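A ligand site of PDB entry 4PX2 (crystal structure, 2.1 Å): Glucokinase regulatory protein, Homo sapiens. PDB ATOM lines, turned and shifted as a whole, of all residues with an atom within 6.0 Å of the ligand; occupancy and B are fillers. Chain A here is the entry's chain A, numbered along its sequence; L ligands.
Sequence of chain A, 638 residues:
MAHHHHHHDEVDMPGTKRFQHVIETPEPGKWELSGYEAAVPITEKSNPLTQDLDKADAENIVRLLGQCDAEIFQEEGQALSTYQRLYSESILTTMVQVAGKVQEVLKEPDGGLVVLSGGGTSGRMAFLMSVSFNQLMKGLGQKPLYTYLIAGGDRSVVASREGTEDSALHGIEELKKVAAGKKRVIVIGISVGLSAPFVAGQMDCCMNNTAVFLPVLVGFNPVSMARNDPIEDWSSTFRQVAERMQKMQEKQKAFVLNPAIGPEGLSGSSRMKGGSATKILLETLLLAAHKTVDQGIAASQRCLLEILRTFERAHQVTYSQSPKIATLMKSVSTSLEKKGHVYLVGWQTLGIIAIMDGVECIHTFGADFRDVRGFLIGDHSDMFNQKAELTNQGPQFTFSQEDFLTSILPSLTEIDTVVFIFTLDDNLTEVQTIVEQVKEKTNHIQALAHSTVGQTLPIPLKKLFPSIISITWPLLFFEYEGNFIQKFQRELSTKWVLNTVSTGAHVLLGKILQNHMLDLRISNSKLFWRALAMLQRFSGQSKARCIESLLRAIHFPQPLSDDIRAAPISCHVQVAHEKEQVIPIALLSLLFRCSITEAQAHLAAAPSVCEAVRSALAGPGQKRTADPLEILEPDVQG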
ATOM      1  N   HIS A  21       8.819  27.283 -30.264  1.00  0.00           N
ATOM      2  CA  HIS A  21       8.555  26.791 -28.901  1.00  0.00           C
ATOM      3  C   HIS A  21       8.835  27.824 -27.788  1.00  0.00           C
ATOM      4  O   HIS A  21       8.368  27.681 -26.652  1.00  0.00           O
ATOM      5  CB  HIS A  21       9.403  25.528 -28.678  1.00  0.00           C
ATOM      6  CG  HIS A  21      10.875  25.819 -28.661  1.00  0.00           C
ATOM      7  ND1 HIS A  21      11.644  25.812 -29.798  1.00  0.00           N
ATOM      8  CD2 HIS A  21      11.693  26.195 -27.652  1.00  0.00           C
ATOM      9  CE1 HIS A  21      12.884  26.160 -29.488  1.00  0.00           C
ATOM     10  NE2 HIS A  21      12.939  26.390 -28.180  1.00  0.00           N
ATOM     11  N   VAL A  22       9.543  28.908 -28.070  1.00  0.00           N
ATOM     12  CA  VAL A  22       9.919  29.803 -26.954  1.00  0.00           C
ATOM     13  C   VAL A  22       8.713  30.563 -26.456  1.00  0.00           C
ATOM     14  O   VAL A  22       8.034  31.097 -27.258  1.00  0.00           O
ATOM     15  CB  VAL A  22      11.050  30.789 -27.359  1.00  0.00           C
ATOM     16  CG1 VAL A  22      11.420  31.723 -26.208  1.00  0.00           C
ATOM     17  CG2 VAL A  22      12.286  30.022 -27.758  1.00  0.00           C
ATOM     18  N   ILE A  23       8.442  30.605 -25.160  1.00  0.00           N
ATOM     19  CA  ILE A  23       7.338  31.420 -24.611  1.00  0.00           C
ATOM     20  C   ILE A  23       7.727  32.918 -24.581  1.00  0.00           C
ATOM     21  O   ILE A  23       8.894  33.246 -24.330  1.00  0.00           O
ATOM     22  CB  ILE A  23       6.967  31.024 -23.147  1.00  0.00           C
ATOM     23  CG1 ILE A  23       6.733  29.508 -22.976  1.00  0.00           C
ATOM     24  CG2 ILE A  23       5.719  31.756 -22.668  1.00  0.00           C
ATOM     25  CD1 ILE A  23       5.732  28.911 -23.938  1.00  0.00           C
ATOM     26  N   TYR A  36       4.043  31.468 -17.995  1.00  0.00           N
ATOM     27  CA  TYR A  36       5.406  31.209 -18.318  1.00  0.00           C
ATOM     28  C   TYR A  36       5.926  30.251 -17.209  1.00  0.00           C
ATOM     29  O   TYR A  36       6.473  29.206 -17.515  1.00  0.00           O
ATOM     30  CB  TYR A  36       6.187  32.504 -18.336  1.00  0.00           C
ATOM     31  CG  TYR A  36       7.606  32.400 -18.776  1.00  0.00           C
ATOM     32  CD1 TYR A  36       8.607  32.030 -17.875  1.00  0.00           C
ATOM     33  CD2 TYR A  36       7.966  32.677 -20.059  1.00  0.00           C
ATOM     34  CE1 TYR A  36       9.947  31.981 -18.250  1.00  0.00           C
ATOM     35  CE2 TYR A  36       9.280  32.608 -20.451  1.00  0.00           C
ATOM     36  CZ  TYR A  36      10.256  32.254 -19.538  1.00  0.00           C
ATOM     37  OH  TYR A  36      11.531  32.171 -19.929  1.00  0.00           O
ATOM     38  N   ALA A  39       5.182  26.619 -17.125  1.00  0.00           N
ATOM     39  CA  ALA A  39       5.868  25.933 -18.162  1.00  0.00           C
ATOM     40  C   ALA A  39       7.370  25.699 -17.894  1.00  0.00           C
ATOM     41  O   ALA A  39       7.982  24.917 -18.623  1.00  0.00           O
ATOM     42  CB  ALA A  39       5.698  26.722 -19.450  1.00  0.00           C
ATOM     43  N   VAL A  40       7.988  26.353 -16.886  1.00  0.00           N
ATOM     44  CA  VAL A  40       9.443  26.185 -16.689  1.00  0.00           C
ATOM     45  C   VAL A  40       9.610  24.806 -16.161  1.00  0.00           C
ATOM     46  O   VAL A  40       9.017  24.476 -15.143  1.00  0.00           O
ATOM     47  CB  VAL A  40      10.066  27.206 -15.695  1.00  0.00           C
ATOM     48  CG1 VAL A  40      11.548  26.890 -15.384  1.00  0.00           C
ATOM     49  CG2 VAL A  40       9.971  28.619 -16.257  1.00  0.00           C
ATOM     50  N   PRO A  41      10.402  23.974 -16.840  1.00  0.00           N
ATOM     51  CA  PRO A  41      10.536  22.647 -16.227  1.00  0.00           C
ATOM     52  C   PRO A  41      11.066  22.694 -14.786  1.00  0.00           C
ATOM     53  O   PRO A  41      11.867  23.593 -14.420  1.00  0.00           O
ATOM     54  CB  PRO A  41      11.430  21.880 -17.193  1.00  0.00           C
ATOM     55  CG  PRO A  41      11.269  22.590 -18.512  1.00  0.00           C
ATOM     56  CD  PRO A  41      11.099  24.041 -18.139  1.00  0.00           C
ATOM     57  N   THR A  43      13.202  21.043 -13.352  1.00  0.00           N
ATOM     58  CA  THR A  43      14.644  20.944 -13.293  1.00  0.00           C
ATOM     59  C   THR A  43      15.312  22.237 -13.699  1.00  0.00           C
ATOM     60  O   THR A  43      16.447  22.374 -13.459  1.00  0.00           O
ATOM     61  CB  THR A  43      15.173  19.819 -14.222  1.00  0.00           C
ATOM     62  OG1 THR A  43      14.765  20.025 -15.583  1.00  0.00           O
ATOM     63  CG2 THR A  43      14.614  18.515 -13.785  1.00  0.00           C
ATOM     64  N   GLU A  44      14.613  23.147 -14.373  1.00  0.00           N
ATOM     65  CA  GLU A  44      15.109  24.426 -14.723  1.00  0.00           C
ATOM     66  C   GLU A  44      14.662  25.491 -13.768  1.00  0.00           C
ATOM     67  O   GLU A  44      15.162  26.552 -13.844  1.00  0.00           O
ATOM     68  CB  GLU A  44      14.658  24.832 -16.148  1.00  0.00           C
ATOM     69  CG  GLU A  44      15.261  23.941 -17.198  1.00  0.00           C
ATOM     70  CD  GLU A  44      16.744  24.152 -17.437  1.00  0.00           C
ATOM     71  OE1 GLU A  44      17.316  25.255 -17.280  1.00  0.00           O
ATOM     72  OE2 GLU A  44      17.378  23.201 -17.779  1.00  0.00           O
ATOM     73  N   GLY A 193      16.460  16.184 -17.004  1.00  0.00           N
ATOM     74  CA  GLY A 193      15.547  17.145 -17.580  1.00  0.00           C
ATOM     75  C   GLY A 193      14.577  16.486 -18.521  1.00  0.00           C
ATOM     76  O   GLY A 193      13.700  17.175 -19.035  1.00  0.00           O
ATOM     77  N   LEU A 194      14.711  15.166 -18.769  1.00  0.00           N
ATOM     78  CA  LEU A 194      14.038  14.481 -19.881  1.00  0.00           C
ATOM     79  C   LEU A 194      14.341  15.379 -21.130  1.00  0.00           C
ATOM     80  O   LEU A 194      13.468  15.967 -21.800  1.00  0.00           O
ATOM     81  CB  LEU A 194      12.520  14.368 -19.643  1.00  0.00           C
ATOM     82  CG  LEU A 194      11.928  13.530 -18.475  1.00  0.00           C
ATOM     83  CD1 LEU A 194      10.407  13.408 -18.571  1.00  0.00           C
ATOM     84  CD2 LEU A 194      12.485  12.123 -18.451  1.00  0.00           C
ATOM     85  N   SER A 195      15.629  15.504 -21.385  1.00  0.00           N
ATOM     86  CA  SER A 195      16.178  16.513 -22.207  1.00  0.00           C
ATOM     87  C   SER A 195      17.143  15.994 -23.284  1.00  0.00           C
ATOM     88  O   SER A 195      17.059  16.464 -24.441  1.00  0.00           O
ATOM     89  CB  SER A 195      16.908  17.498 -21.319  1.00  0.00           C
ATOM     90  OG  SER A 195      17.895  18.161 -22.040  1.00  0.00           O
ATOM     91  N   ASN A 221      11.349  15.390 -14.398  1.00  0.00           N
ATOM     92  CA  ASN A 221      10.282  16.280 -14.819  1.00  0.00           C
ATOM     93  C   ASN A 221       9.077  15.441 -15.198  1.00  0.00           C
ATOM     94  O   ASN A 221       9.227  14.336 -15.661  1.00  0.00           O
ATOM     95  CB  ASN A 221      10.704  17.085 -16.024  1.00  0.00           C
ATOM     96  CG  ASN A 221      11.518  18.295 -15.694  1.00  0.00           C
ATOM     97  OD1 ASN A 221      11.226  18.997 -14.738  1.00  0.00           O
ATOM     98  ND2 ASN A 221      12.549  18.547 -16.485  1.00  0.00           N
ATOM     99  N   MET A 225       6.618  18.318 -19.206  1.00  0.00           N
ATOM    100  CA  MET A 225       7.673  19.322 -19.231  1.00  0.00           C
ATOM    101  C   MET A 225       8.910  18.869 -19.939  1.00  0.00           C
ATOM    102  O   MET A 225       9.930  19.540 -19.854  1.00  0.00           O
ATOM    103  CB  MET A 225       8.051  19.698 -17.813  1.00  0.00           C
ATOM    104  CG  MET A 225       7.141  20.755 -17.236  1.00  0.00           C
ATOM    105  SD  MET A 225       7.286  20.657 -15.452  1.00  0.00           S
ATOM    106  CE  MET A 225       6.475  22.168 -14.951  1.00  0.00           C
ATOM    107  N   ALA A 226       8.875  17.697 -20.532  1.00  0.00           N
ATOM    108  CA  ALA A 226      10.020  17.213 -21.264  1.00  0.00           C
ATOM    109  C   ALA A 226      10.316  18.149 -22.419  1.00  0.00           C
ATOM    110  O   ALA A 226       9.396  18.805 -22.870  1.00  0.00           O
ATOM    111  CB  ALA A 226       9.718  15.864 -21.812  1.00  0.00           C
ATOM    112  N   ARG A 227      11.569  18.199 -22.891  1.00  0.00           N
ATOM    113  CA  ARG A 227      11.899  19.016 -24.055  1.00  0.00           C
ATOM    114  C   ARG A 227      11.052  18.718 -25.276  1.00  0.00           C
ATOM    115  O   ARG A 227      10.835  17.539 -25.668  1.00  0.00           O
ATOM    116  CB  ARG A 227      13.377  18.912 -24.390  1.00  0.00           C
ATOM    117  CG  ARG A 227      14.184  19.692 -23.376  1.00  0.00           C
ATOM    118  CD  ARG A 227      15.611  19.832 -23.598  1.00  0.00           C
ATOM    119  NE  ARG A 227      15.954  20.473 -24.870  1.00  0.00           N
ATOM    120  CZ  ARG A 227      17.194  20.474 -25.341  1.00  0.00           C
ATOM    121  NH1 ARG A 227      18.144  19.874 -24.612  1.00  0.00           N
ATOM    122  NH2 ARG A 227      17.493  21.025 -26.522  1.00  0.00           N
ATOM    123  N   ASN A 228      10.612  19.812 -25.909  1.00  0.00           N
ATOM    124  CA  ASN A 228       9.837  19.753 -27.112  1.00  0.00           C
ATOM    125  C   ASN A 228      10.419  20.599 -28.240  1.00  0.00           C
ATOM    126  O   ASN A 228       9.703  20.924 -29.095  1.00  0.00           O
ATOM    127  CB  ASN A 228       8.391  20.176 -26.802  1.00  0.00           C
ATOM    128  CG  ASN A 228       7.376  19.609 -27.783  1.00  0.00           C
ATOM    129  OD1 ASN A 228       7.432  18.446 -28.197  1.00  0.00           O
ATOM    130  ND2 ASN A 228       6.403  20.445 -28.138  1.00  0.00           N
ATOM    131  N   ASP A 229      11.699  20.916 -28.241  1.00  0.00           N
ATOM    132  CA  ASP A 229      12.367  21.588 -29.346  1.00  0.00           C
ATOM    133  C   ASP A 229      12.922  20.534 -30.261  1.00  0.00           C
ATOM    134  O   ASP A 229      13.183  19.424 -29.812  1.00  0.00           O
ATOM    135  CB  ASP A 229      13.498  22.560 -28.866  1.00  0.00           C
ATOM    136  CG  ASP A 229      14.614  21.885 -28.017  1.00  0.00           C
ATOM    137  OD1 ASP A 229      14.247  21.243 -26.998  1.00  0.00           O
ATOM    138  OD2 ASP A 229      15.851  22.106 -28.239  1.00  0.00           O
ATOM    139  N   ARG A 239       9.765  14.958 -25.618  1.00  0.00           N
ATOM    140  CA  ARG A 239       8.376  14.878 -25.144  1.00  0.00           C
ATOM    141  C   ARG A 239       7.550  13.829 -25.842  1.00  0.00           C
ATOM    142  O   ARG A 239       6.775  13.129 -25.207  1.00  0.00           O
ATOM    143  CB  ARG A 239       7.699  16.220 -25.289  1.00  0.00           C
ATOM    144  CG  ARG A 239       6.414  16.356 -24.501  1.00  0.00           C
ATOM    145  CD  ARG A 239       6.531  17.610 -23.673  1.00  0.00           C
ATOM    146  NE  ARG A 239       5.745  18.675 -24.135  1.00  0.00           N
ATOM    147  CZ  ARG A 239       5.956  19.962 -23.888  1.00  0.00           C
ATOM    148  NH1 ARG A 239       7.024  20.447 -23.257  1.00  0.00           N
ATOM    149  NH2 ARG A 239       5.059  20.796 -24.357  1.00  0.00           N
ATOM    150  N   LYS A 526      20.605  22.671 -24.672  1.00  0.00           N
ATOM    151  CA  LYS A 526      19.942  22.988 -23.382  1.00  0.00           C
ATOM    152  C   LYS A 526      20.471  24.255 -22.750  1.00  0.00           C
ATOM    153  O   LYS A 526      19.704  25.117 -22.333  1.00  0.00           O
ATOM    154  CB  LYS A 526      20.137  21.798 -22.410  1.00  0.00           C
ATOM    155  CG  LYS A 526      19.537  21.974 -21.050  1.00  0.00           C
ATOM    156  CD  LYS A 526      19.567  20.666 -20.192  1.00  0.00           C
ATOM    157  CE  LYS A 526      20.974  20.246 -19.840  1.00  0.00           C
ATOM    158  NZ  LYS A 526      20.803  18.867 -19.368  1.00  0.00           N
ATOM    159  N   TRP A 529      19.202  27.346 -24.406  1.00  0.00           N
ATOM    160  CA  TRP A 529      17.886  27.703 -23.899  1.00  0.00           C
ATOM    161  C   TRP A 529      17.932  28.283 -22.537  1.00  0.00           C
ATOM    162  O   TRP A 529      17.153  29.187 -22.244  1.00  0.00           O
ATOM    163  CB  TRP A 529      16.849  26.533 -23.974  1.00  0.00           C
ATOM    164  CG  TRP A 529      16.725  25.981 -25.363  1.00  0.00           C
ATOM    165  CD1 TRP A 529      16.971  24.720 -25.752  1.00  0.00           C
ATOM    166  CD2 TRP A 529      16.403  26.720 -26.544  1.00  0.00           C
ATOM    167  NE1 TRP A 529      16.776  24.593 -27.126  1.00  0.00           N
ATOM    168  CE2 TRP A 529      16.451  25.805 -27.628  1.00  0.00           C
ATOM    169  CE3 TRP A 529      16.042  28.034 -26.802  1.00  0.00           C
ATOM    170  CZ2 TRP A 529      16.126  26.178 -28.960  1.00  0.00           C
ATOM    171  CZ3 TRP A 529      15.720  28.410 -28.171  1.00  0.00           C
ATOM    172  CH2 TRP A 529      15.831  27.498 -29.188  1.00  0.00           C
ATOM    173  N   ARG A 530      18.824  27.758 -21.675  1.00  0.00           N
ATOM    174  CA  ARG A 530      18.952  28.263 -20.319  1.00  0.00           C
ATOM    175  C   ARG A 530      19.441  29.705 -20.401  1.00  0.00           C
ATOM    176  O   ARG A 530      18.913  30.593 -19.696  1.00  0.00           O
ATOM    177  CB  ARG A 530      19.863  27.377 -19.446  1.00  0.00           C
ATOM    178  CG  ARG A 530      19.912  27.781 -17.977  1.00  0.00           C
ATOM    179  CD  ARG A 530      20.648  26.751 -17.140  1.00  0.00           C
ATOM    180  NE  ARG A 530      20.110  25.381 -17.326  1.00  0.00           N
ATOM    181  CZ  ARG A 530      20.806  24.264 -17.167  1.00  0.00           C
ATOM    182  NH1 ARG A 530      22.069  24.354 -16.846  1.00  0.00           N
ATOM    183  NH2 ARG A 530      20.281  23.049 -17.399  1.00  0.00           N
ATOM    184  N   LEU A 532      18.990  31.888 -22.907  1.00  0.00           N
ATOM    185  CA  LEU A 532      17.869  32.683 -23.381  1.00  0.00           C
ATOM    186  C   LEU A 532      16.856  32.898 -22.271  1.00  0.00           C
ATOM    187  O   LEU A 532      16.426  34.020 -22.063  1.00  0.00           O
ATOM    188  CB  LEU A 532      17.225  32.073 -24.622  1.00  0.00           C
ATOM    189  CG  LEU A 532      15.962  32.772 -25.073  1.00  0.00           C
ATOM    190  CD1 LEU A 532      16.335  34.191 -25.434  1.00  0.00           C
ATOM    191  CD2 LEU A 532      15.308  32.027 -26.272  1.00  0.00           C
ATOM    192  N   ALA A 533      16.460  31.855 -21.559  1.00  0.00           N
ATOM    193  CA  ALA A 533      15.562  32.040 -20.398  1.00  0.00           C
ATOM    194  C   ALA A 533      16.095  33.032 -19.360  1.00  0.00           C
ATOM    195  O   ALA A 533      15.376  33.871 -18.805  1.00  0.00           O
ATOM    196  CB  ALA A 533      15.266  30.701 -19.706  1.00  0.00           C
ATOM    197  N   GLN A 536      15.642  36.660 -20.648  1.00  0.00           N
ATOM    198  CA  GLN A 536      14.278  37.087 -20.364  1.00  0.00           C
ATOM    199  C   GLN A 536      14.062  37.384 -18.857  1.00  0.00           C
ATOM    200  O   GLN A 536      13.396  38.332 -18.507  1.00  0.00           O
ATOM    201  CB  GLN A 536      13.237  36.048 -20.797  1.00  0.00           C
ATOM    202  CG  GLN A 536      13.299  35.569 -22.244  1.00  0.00           C
ATOM    203  CD  GLN A 536      12.286  34.447 -22.488  1.00  0.00           C
ATOM    204  OE1 GLN A 536      12.517  33.310 -22.101  1.00  0.00           O
ATOM    205  NE2 GLN A 536      11.128  34.784 -23.026  1.00  0.00           N
HETATM  206  C1  LIG L   1      11.619  24.977 -21.589  1.00  0.00           C
HETATM  207  C2  LIG L   1      11.378  26.103 -20.922  1.00  0.00           C
HETATM  208  C3  LIG L   1      10.162  26.805 -20.750  1.00  0.00           C
HETATM  209  C4  LIG L   1      10.203  27.962 -19.950  1.00  0.00           C
HETATM  210  C5  LIG L   1      11.441  28.331 -19.361  1.00  0.00           C
HETATM  211  C6  LIG L   1      12.649  27.625 -19.505  1.00  0.00           C
HETATM  212  C7  LIG L   1      12.581  26.503 -20.304  1.00  0.00           C
HETATM  213  O1  LIG L   1      13.531  25.604 -20.651  1.00  0.00           O
HETATM  214  C8  LIG L   1      12.890  24.670 -21.469  1.00  0.00           C
HETATM  215  C9  LIG L   1      13.534  23.459 -22.154  1.00  0.00           C
HETATM  216  C10 LIG L   1      13.845  22.290 -21.194  1.00  0.00           C
HETATM  217  C11 LIG L   1      12.882  21.243 -20.986  1.00  0.00           C
HETATM  218  C12 LIG L   1      13.085  20.119 -20.154  1.00  0.00           C
HETATM  219  C13 LIG L   1      14.364  20.063 -19.550  1.00  0.00           C
HETATM  220  C14 LIG L   1      15.311  21.064 -19.744  1.00  0.00           C
HETATM  221  C15 LIG L   1      15.089  22.182 -20.565  1.00  0.00           C
HETATM  222  N1  LIG L   1      12.601  22.889 -23.194  1.00  0.00           N
HETATM  223  S1  LIG L   1      12.333  23.507 -24.768  1.00  0.00           S
HETATM  224  O2  LIG L   1      13.502  23.185 -25.657  1.00  0.00           O
HETATM  225  O3  LIG L   1      11.117  22.789 -25.222  1.00  0.00           O
HETATM  226  C16 LIG L   1      11.947  25.269 -24.564  1.00  0.00           C
HETATM  227  C17 LIG L   1      12.980  26.221 -24.502  1.00  0.00           C
HETATM  228  C18 LIG L   1      12.679  27.551 -24.284  1.00  0.00           C
HETATM  229  O4  LIG L   1      13.810  28.343 -24.288  1.00  0.00           O
HETATM  230  C19 LIG L   1      14.047  29.250 -23.173  1.00  0.00           C
HETATM  231  C20 LIG L   1      13.006  30.375 -22.840  1.00  0.00           C
HETATM  232  C21 LIG L   1      11.529  29.861 -22.682  1.00  0.00           C
HETATM  233  O5  LIG L   1      10.914  29.290 -23.909  1.00  0.00           O
HETATM  234  C22 LIG L   1      11.340  27.973 -24.119  1.00  0.00           C
HETATM  235  C23 LIG L   1      10.280  27.046 -24.179  1.00  0.00           C
HETATM  236  C24 LIG L   1      10.600  25.693 -24.394  1.00  0.00           C
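O2 of the ligand sits close to OD1 of Asp 229 (2.5 Å). The backbone NH of Ile 23 sits at hydrogen-bond distance from an oxygen (O5) of the ligand (3.1 Å). The backbone NH (N) of Asn 228 is in hydrogen-bond range of an oxygen (O3) of the ligand (3.1 Å).
The side-chain carboxylate (OD2) of Asp 229 lies within salt-bridge range of the guanidinium group (NH2) of Arg 227 (2.6 Å). The side-chain carboxylate of Asp 229 is in hydrogen-bond range of the indole nitrogen of Trp 529, 2.9 Å away. ND2 of Asn 221 sits at hydrogen-bond distance from O of Gly 193. The backbone carbonyl oxygen of Ile 23 is in hydrogen-bond range of the side-chain amide nitrogen of Gln 536, at 3.0 Å. The side-chain hydroxyl of Tyr 36 lies within hydrogen-bond range of the side-chain amide oxygen of Gln 536, at 2.6 Å. OG of Ser 195 sits at hydrogen-bond distance from NH1 of Arg 227. O of Leu 194 is in hydrogen-bond range of N of Arg 227. The guanidinium group (NE) of Arg 530 is in salt-bridge range of the side-chain carboxylate (OE1) of Glu 44, at 2.8 Å.
Residues that only touch the ligand: His 21, Val 22, Tyr 36, Ala 39, Val 40, Pro 41, Thr 43, Glu 44, Gly 193, Asn 221, Met 225, Arg 227, Trp 529, Ala 533 and Gln 536. Hydrophobic or aromatic side chains within 4 Å of the ligand: His 21, Val 22, Val 40, Pro 41, Trp 529 and Ala 533. Within 4 Å of the ligand: His 21, Val 22, Ile 23, Tyr 36, Ala 39, Val 40, Pro 41, Thr 43, Glu 44, Gly 193, Asn 221, Met 225, Arg 227, Asn 228, Asp 229, Trp 529, Ala 533 and Gln 536. Along chain A the residues within 4 Å of the ligand span positions 21 to 536. The nearest printed residue that does not touch the ligand is Ser 195 (4.02 Å).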
